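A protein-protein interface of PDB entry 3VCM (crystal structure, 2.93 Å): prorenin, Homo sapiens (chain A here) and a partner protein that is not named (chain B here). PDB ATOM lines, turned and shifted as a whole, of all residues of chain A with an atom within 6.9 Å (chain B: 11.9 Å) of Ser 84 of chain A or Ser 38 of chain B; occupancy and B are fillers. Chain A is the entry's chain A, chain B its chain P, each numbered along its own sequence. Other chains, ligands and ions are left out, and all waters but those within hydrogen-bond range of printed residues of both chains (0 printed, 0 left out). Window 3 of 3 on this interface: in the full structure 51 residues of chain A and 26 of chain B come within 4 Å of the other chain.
The backbone NH of Thr 85 of chain A sits close to the backbone carbonyl oxygen of Ser 38 of chain B.
O of Thr 85 of chain A lies close to SD of Met 41 of chain B, at 3.3 Å.
The backbone NH of Thr 2 of chain A sits at hydrogen-bond distance from the backbone carbonyl oxygen of Arg 82 of chain A (2.8 Å).
OE1 of Gln 39 of chain B sits close to O of Arg 43 of chain B (3.0 Å).
OE1 of Gln 39 of chain B touches CG2 of Thr 2 of chain A, 3.5 Å away.
Thr 2 of chain A touches Arg 43 of chain B (N to O, 3.6 Å).
Tyr 83 of chain A touches Gln 39 of chain B.
CG of Tyr 83 of chain A touches CG of Met 41 of chain B, 3.5 Å away.
Arg 43 of chain B touches Tyr 83 of chain A (O to CD1, 3.2 Å).
Ser 84 of chain A touches Ser 38 of chain B (CB to N, 3.8 Å).
CG of Gln 39 of chain B touches CB of Ser 84 of chain A (3.5 Å).
Leu 117 of chain A touches Met 41 of chain B.
Ser 84 of chain A touches just these residues of chain B: Ser 38 (3.8 Å) and Gln 39 (3.5 Å).
No residue of chain B comes within 4 Å of Arg 82 of chain A.
No residue of chain B comes within 4 Å of Gly 86 of chain A.
Of the printed residues of chain A, Met 41 of chain B touches Tyr 83 (3.5 Å), Thr 85 (3.3 Å) and Leu 117 (3.2 Å).
Of the printed residues of chain B, Thr 85 of chain A touches Ser 38 (2.4 Å) and Met 41 (3.3 Å).
Ala 31 of chain B touches none of the printed residues of chain A.
Gly 34 of chain B touches none of the printed residues of chain A.
The nearest residue of chain B that does not touch Ser 84 of chain A is Trp 37 of chain B (4.2 Å).
The nearest residue of chain A that does not touch Ser 38 of chain B is Gly 86 of chain A (4.5 Å).
Of the 8 printed residues of chain A, 5 touch a printed residue of chain B.
Printed residues of chain A that touch a printed residue of chain B: Thr 2, Tyr 83, Ser 84, Thr 85 and Leu 117.
Hydrophobic or aromatic side chains of chain A that line the printed part of chain B: Tyr 83.
Of the 14 printed residues of chain B, 4 touch a printed residue of chain A.
Along chain B the printed residues that touch a printed residue of chain A span positions 38 to 43.
Among the printed residues, no Asp or Glu carboxylate lies within 4 Å of a Lys or Arg side-chain nitrogen of the other chain.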
ATOM      1  N   THR A   2      -1.957  26.340   7.382  1.00  0.00           N
ATOM      2  CA  THR A   2      -1.314  27.581   6.928  1.00  0.00           C
ATOM      3  C   THR A   2      -0.613  28.224   8.121  1.00  0.00           C
ATOM      4  O   THR A   2      -1.205  28.284   9.197  1.00  0.00           O
ATOM      5  CB  THR A   2      -2.309  28.594   6.257  1.00  0.00           C
ATOM      6  OG1 THR A   2      -3.184  29.191   7.220  1.00  0.00           O
ATOM      7  CG2 THR A   2      -3.112  27.992   5.107  1.00  0.00           C
ATOM      8  N   ARG A  82      -3.503  26.129  12.432  1.00  0.00           N
ATOM      9  CA  ARG A  82      -4.183  27.257  11.795  1.00  0.00           C
ATOM     10  C   ARG A  82      -4.503  27.008  10.327  1.00  0.00           C
ATOM     11  O   ARG A  82      -3.640  26.588   9.563  1.00  0.00           O
ATOM     12  CB  ARG A  82      -3.359  28.548  11.943  1.00  0.00           C
ATOM     13  CG  ARG A  82      -4.098  29.784  11.490  1.00  0.00           C
ATOM     14  CD  ARG A  82      -3.179  30.865  10.977  1.00  0.00           C
ATOM     15  NE  ARG A  82      -3.953  31.875  10.257  1.00  0.00           N
ATOM     16  CZ  ARG A  82      -3.455  33.005   9.767  1.00  0.00           C
ATOM     17  NH1 ARG A  82      -4.243  33.860   9.126  1.00  0.00           N
ATOM     18  NH2 ARG A  82      -2.168  33.294   9.918  1.00  0.00           N
ATOM     19  N   TYR A  83      -5.748  27.301   9.939  1.00  0.00           N
ATOM     20  CA  TYR A  83      -6.229  27.226   8.558  1.00  0.00           C
ATOM     21  C   TYR A  83      -6.771  28.622   8.211  1.00  0.00           C
ATOM     22  O   TYR A  83      -6.747  29.500   9.085  1.00  0.00           O
ATOM     23  CB  TYR A  83      -7.300  26.126   8.423  1.00  0.00           C
ATOM     24  CG  TYR A  83      -6.770  24.740   8.734  1.00  0.00           C
ATOM     25  CD1 TYR A  83      -6.125  23.982   7.757  1.00  0.00           C
ATOM     26  CD2 TYR A  83      -6.919  24.177  10.001  1.00  0.00           C
ATOM     27  CE1 TYR A  83      -5.622  22.710   8.037  1.00  0.00           C
ATOM     28  CE2 TYR A  83      -6.416  22.905  10.293  1.00  0.00           C
ATOM     29  CZ  TYR A  83      -5.772  22.177   9.304  1.00  0.00           C
ATOM     30  OH  TYR A  83      -5.288  20.924   9.572  1.00  0.00           O
ATOM     31  N   SER A  84      -7.227  28.852   6.957  1.00  0.00           N
ATOM     32  CA  SER A  84      -7.789  30.150   6.544  1.00  0.00           C
ATOM     33  C   SER A  84      -8.972  30.523   7.450  1.00  0.00           C
ATOM     34  O   SER A  84      -9.123  31.687   7.814  1.00  0.00           O
ATOM     35  CB  SER A  84      -8.219  30.116   5.084  1.00  0.00           C
ATOM     36  OG  SER A  84      -7.965  31.348   4.430  1.00  0.00           O
ATOM     37  N   THR A  85      -9.785  29.501   7.828  1.00  0.00           N
ATOM     38  CA  THR A  85     -10.887  29.482   8.811  1.00  0.00           C
ATOM     39  C   THR A  85     -11.409  28.054   9.093  1.00  0.00           C
ATOM     40  O   THR A  85     -11.994  27.425   8.211  1.00  0.00           O
ATOM     41  CB  THR A  85     -11.975  30.571   8.641  1.00  0.00           C
ATOM     42  OG1 THR A  85     -13.096  30.231   9.463  1.00  0.00           O
ATOM     43  CG2 THR A  85     -12.433  30.764   7.201  1.00  0.00           C
ATOM     44  N   GLY A  86     -11.207  27.539  10.300  1.00  0.00           N
ATOM     45  CA  GLY A  86     -10.566  28.245  11.388  1.00  0.00           C
ATOM     46  C   GLY A  86      -9.371  27.524  11.960  1.00  0.00           C
ATOM     47  O   GLY A  86      -8.254  27.682  11.457  1.00  0.00           O
ATOM     48  N   THR A  87      -9.589  26.738  13.028  1.00  0.00           N
ATOM     49  CA  THR A  87      -8.477  26.119  13.729  1.00  0.00           C
ATOM     50  C   THR A  87      -8.746  24.718  14.289  1.00  0.00           C
ATOM     51  O   THR A  87      -9.903  24.341  14.508  1.00  0.00           O
ATOM     52  CB  THR A  87      -7.983  27.142  14.794  1.00  0.00           C
ATOM     53  OG1 THR A  87      -6.562  27.228  14.792  1.00  0.00           O
ATOM     54  CG2 THR A  87      -8.537  26.900  16.191  1.00  0.00           C
ATOM     55  N   LEU A 117     -17.261  20.541   9.663  1.00  0.00           N
ATOM     56  CA  LEU A 117     -16.612  20.907   8.381  1.00  0.00           C
ATOM     57  C   LEU A 117     -15.095  21.071   8.359  1.00  0.00           C
ATOM     58  O   LEU A 117     -14.589  22.108   8.786  1.00  0.00           O
ATOM     59  CB  LEU A 117     -17.340  21.960   7.514  1.00  0.00           C
ATOM     60  CG  LEU A 117     -16.789  22.187   6.084  1.00  0.00           C
ATOM     61  CD1 LEU A 117     -17.331  21.159   5.087  1.00  0.00           C
ATOM     62  CD2 LEU A 117     -17.067  23.600   5.603  1.00  0.00           C
ATOM     63  N   MET B  30     -20.557  20.479  -4.115  1.00  0.00           N
ATOM     64  CA  MET B  30     -19.167  20.892  -3.896  1.00  0.00           C
ATOM     65  C   MET B  30     -18.927  22.388  -3.952  1.00  0.00           C
ATOM     66  O   MET B  30     -18.082  22.887  -3.213  1.00  0.00           O
ATOM     67  CB  MET B  30     -18.216  20.168  -4.857  1.00  0.00           C
ATOM     68  CG  MET B  30     -17.928  18.739  -4.463  1.00  0.00           C
ATOM     69  SD  MET B  30     -17.117  18.597  -2.857  1.00  0.00           S
ATOM     70  CE  MET B  30     -18.423  17.899  -1.935  1.00  0.00           C
ATOM     71  N   ALA B  31     -19.668  23.100  -4.821  1.00  0.00           N
ATOM     72  CA  ALA B  31     -19.567  24.552  -4.979  1.00  0.00           C
ATOM     73  C   ALA B  31     -20.170  25.286  -3.780  1.00  0.00           C
ATOM     74  O   ALA B  31     -19.741  26.400  -3.466  1.00  0.00           O
ATOM     75  CB  ALA B  31     -20.264  24.988  -6.256  1.00  0.00           C
ATOM     76  N   ARG B  32     -21.157  24.651  -3.111  1.00  0.00           N
ATOM     77  CA  ARG B  32     -21.875  25.194  -1.953  1.00  0.00           C
ATOM     78  C   ARG B  32     -21.222  24.883  -0.581  1.00  0.00           C
ATOM     79  O   ARG B  32     -21.922  24.783   0.429  1.00  0.00           O
ATOM     80  CB  ARG B  32     -23.373  24.800  -2.001  1.00  0.00           C
ATOM     81  CG  ARG B  32     -24.172  25.426  -3.152  1.00  0.00           C
ATOM     82  CD  ARG B  32     -24.517  26.900  -2.938  1.00  0.00           C
ATOM     83  NE  ARG B  32     -24.837  27.571  -4.198  1.00  0.00           N
ATOM     84  CZ  ARG B  32     -23.968  28.217  -4.977  1.00  0.00           C
ATOM     85  NH1 ARG B  32     -22.684  28.288  -4.612  1.00  0.00           N
ATOM     86  NH2 ARG B  32     -24.352  28.788  -6.100  1.00  0.00           N
ATOM     87  N   LEU B  33     -19.875  24.773  -0.549  1.00  0.00           N
ATOM     88  CA  LEU B  33     -19.095  24.518   0.674  1.00  0.00           C
ATOM     89  C   LEU B  33     -18.405  25.789   1.210  1.00  0.00           C
ATOM     90  O   LEU B  33     -17.781  25.755   2.275  1.00  0.00           O
ATOM     91  CB  LEU B  33     -18.052  23.399   0.465  1.00  0.00           C
ATOM     92  CG  LEU B  33     -18.542  21.965   0.227  1.00  0.00           C
ATOM     93  CD1 LEU B  33     -17.371  21.065  -0.038  1.00  0.00           C
ATOM     94  CD2 LEU B  33     -19.324  21.417   1.413  1.00  0.00           C
ATOM     95  N   GLY B  34     -18.533  26.889   0.468  1.00  0.00           N
ATOM     96  CA  GLY B  34     -17.946  28.176   0.826  1.00  0.00           C
ATOM     97  C   GLY B  34     -16.942  28.677  -0.196  1.00  0.00           C
ATOM     98  O   GLY B  34     -16.590  27.938  -1.121  1.00  0.00           O
ATOM     99  N   PRO B  35     -16.447  29.930  -0.052  1.00  0.00           N
ATOM    100  CA  PRO B  35     -15.486  30.471  -1.043  1.00  0.00           C
ATOM    101  C   PRO B  35     -14.110  29.795  -1.052  1.00  0.00           C
ATOM    102  O   PRO B  35     -13.857  28.938  -0.205  1.00  0.00           O
ATOM    103  CB  PRO B  35     -15.402  31.955  -0.685  1.00  0.00           C
ATOM    104  CG  PRO B  35     -15.830  32.039   0.725  1.00  0.00           C
ATOM    105  CD  PRO B  35     -16.766  30.917   0.999  1.00  0.00           C
ATOM    106  N   GLU B  36     -13.233  30.154  -2.031  1.00  0.00           N
ATOM    107  CA  GLU B  36     -11.873  29.603  -2.195  1.00  0.00           C
ATOM    108  C   GLU B  36     -11.079  29.733  -0.893  1.00  0.00           C
ATOM    109  O   GLU B  36     -10.499  28.748  -0.426  1.00  0.00           O
ATOM    110  CB  GLU B  36     -11.136  30.264  -3.375  1.00  0.00           C
ATOM    111  CG  GLU B  36     -11.526  29.717  -4.738  1.00  0.00           C
ATOM    112  CD  GLU B  36     -11.060  28.300  -5.018  1.00  0.00           C
ATOM    113  OE1 GLU B  36     -11.890  27.370  -4.899  1.00  0.00           O
ATOM    114  OE2 GLU B  36      -9.861  28.117  -5.333  1.00  0.00           O
ATOM    115  N   TRP B  37     -11.107  30.938  -0.287  1.00  0.00           N
ATOM    116  CA  TRP B  37     -10.550  31.179   1.035  1.00  0.00           C
ATOM    117  C   TRP B  37     -11.634  30.584   1.948  1.00  0.00           C
ATOM    118  O   TRP B  37     -12.804  30.910   1.760  1.00  0.00           O
ATOM    119  CB  TRP B  37     -10.365  32.698   1.304  1.00  0.00           C
ATOM    120  CG  TRP B  37     -11.645  33.495   1.338  1.00  0.00           C
ATOM    121  CD1 TRP B  37     -12.280  34.069   0.278  1.00  0.00           C
ATOM    122  CD2 TRP B  37     -12.487  33.725   2.484  1.00  0.00           C
ATOM    123  NE1 TRP B  37     -13.464  34.645   0.687  1.00  0.00           N
ATOM    124  CE2 TRP B  37     -13.618  34.444   2.035  1.00  0.00           C
ATOM    125  CE3 TRP B  37     -12.416  33.355   3.841  1.00  0.00           C
ATOM    126  CZ2 TRP B  37     -14.654  34.828   2.899  1.00  0.00           C
ATOM    127  CZ3 TRP B  37     -13.441  33.738   4.694  1.00  0.00           C
ATOM    128  CH2 TRP B  37     -14.548  34.455   4.220  1.00  0.00           C
ATOM    129  N   SER B  38     -11.291  29.650   2.837  1.00  0.00           N
ATOM    130  CA  SER B  38     -12.242  29.049   3.782  1.00  0.00           C
ATOM    131  C   SER B  38     -11.656  28.006   4.722  1.00  0.00           C
ATOM    132  O   SER B  38     -11.770  28.214   5.913  1.00  0.00           O
ATOM    133  CB  SER B  38     -13.543  28.569   3.138  1.00  0.00           C
ATOM    134  OG  SER B  38     -14.540  29.575   3.194  1.00  0.00           O
ATOM    135  N   GLN B  39     -11.013  26.915   4.275  1.00  0.00           N
ATOM    136  CA  GLN B  39     -10.751  26.427   2.928  1.00  0.00           C
ATOM    137  C   GLN B  39     -11.012  24.927   3.148  1.00  0.00           C
ATOM    138  O   GLN B  39     -10.040  24.237   3.482  1.00  0.00           O
ATOM    139  CB  GLN B  39      -9.271  26.703   2.537  1.00  0.00           C
ATOM    140  CG  GLN B  39      -8.305  26.830   3.754  1.00  0.00           C
ATOM    141  CD  GLN B  39      -7.037  26.007   3.762  1.00  0.00           C
ATOM    142  OE1 GLN B  39      -6.121  26.289   4.535  1.00  0.00           O
ATOM    143  NE2 GLN B  39      -6.946  24.966   2.934  1.00  0.00           N
ATOM    144  N   PRO B  40     -12.287  24.421   3.214  1.00  0.00           N
ATOM    145  CA  PRO B  40     -12.532  23.002   3.556  1.00  0.00           C
ATOM    146  C   PRO B  40     -11.346  22.067   3.907  1.00  0.00           C
ATOM    147  O   PRO B  40     -11.078  21.055   3.257  1.00  0.00           O
ATOM    148  CB  PRO B  40     -13.486  22.572   2.454  1.00  0.00           C
ATOM    149  CG  PRO B  40     -14.175  23.970   1.965  1.00  0.00           C
ATOM    150  CD  PRO B  40     -13.562  25.043   2.810  1.00  0.00           C
ATOM    151  N   MET B  41     -10.654  22.486   4.991  1.00  0.00           N
ATOM    152  CA  MET B  41      -9.448  21.994   5.674  1.00  0.00           C
ATOM    153  C   MET B  41      -8.683  20.825   5.080  1.00  0.00           C
ATOM    154  O   MET B  41      -9.211  19.710   5.017  1.00  0.00           O
ATOM    155  CB  MET B  41      -9.703  21.834   7.175  1.00  0.00           C
ATOM    156  CG  MET B  41      -9.760  23.151   7.952  1.00  0.00           C
ATOM    157  SD  MET B  41     -10.731  24.539   7.279  1.00  0.00           S
ATOM    158  CE  MET B  41     -12.355  23.995   7.607  1.00  0.00           C
ATOM    159  N   LYS B  42      -7.423  21.085   4.668  1.00  0.00           N
ATOM    160  CA  LYS B  42      -6.505  20.083   4.093  1.00  0.00           C
ATOM    161  C   LYS B  42      -5.036  20.508   4.001  1.00  0.00           C
ATOM    162  O   LYS B  42      -4.177  19.655   3.789  1.00  0.00           O
ATOM    163  CB  LYS B  42      -7.008  19.496   2.743  1.00  0.00           C
ATOM    164  CG  LYS B  42      -7.175  20.486   1.601  1.00  0.00           C
ATOM    165  CD  LYS B  42      -7.944  19.858   0.446  1.00  0.00           C
ATOM    166  CE  LYS B  42      -8.350  20.914  -0.556  1.00  0.00           C
ATOM    167  NZ  LYS B  42      -8.317  20.413  -1.948  1.00  0.00           N
ATOM    168  N   ARG B  43      -4.740  21.813   4.154  1.00  0.00           N
ATOM    169  CA  ARG B  43      -3.378  22.324   4.007  1.00  0.00           C
ATOM    170  C   ARG B  43      -3.121  23.623   4.760  1.00  0.00           C
ATOM    171  O   ARG B  43      -4.037  24.243   5.284  1.00  0.00           O
ATOM    172  CB  ARG B  43      -3.040  22.456   2.502  1.00  0.00           C
ATOM    173  CG  ARG B  43      -2.716  23.859   1.973  1.00  0.00           C
ATOM    174  CD  ARG B  43      -1.230  24.012   1.665  1.00  0.00           C
ATOM    175  NE  ARG B  43      -0.399  23.453   2.727  1.00  0.00           N
ATOM    176  CZ  ARG B  43      -0.034  24.101   3.825  1.00  0.00           C
ATOM    177  NH1 ARG B  43      -0.402  25.363   4.016  1.00  0.00           N
ATOM    178  NH2 ARG B  43       0.690  23.488   4.751  1.00  0.00           N
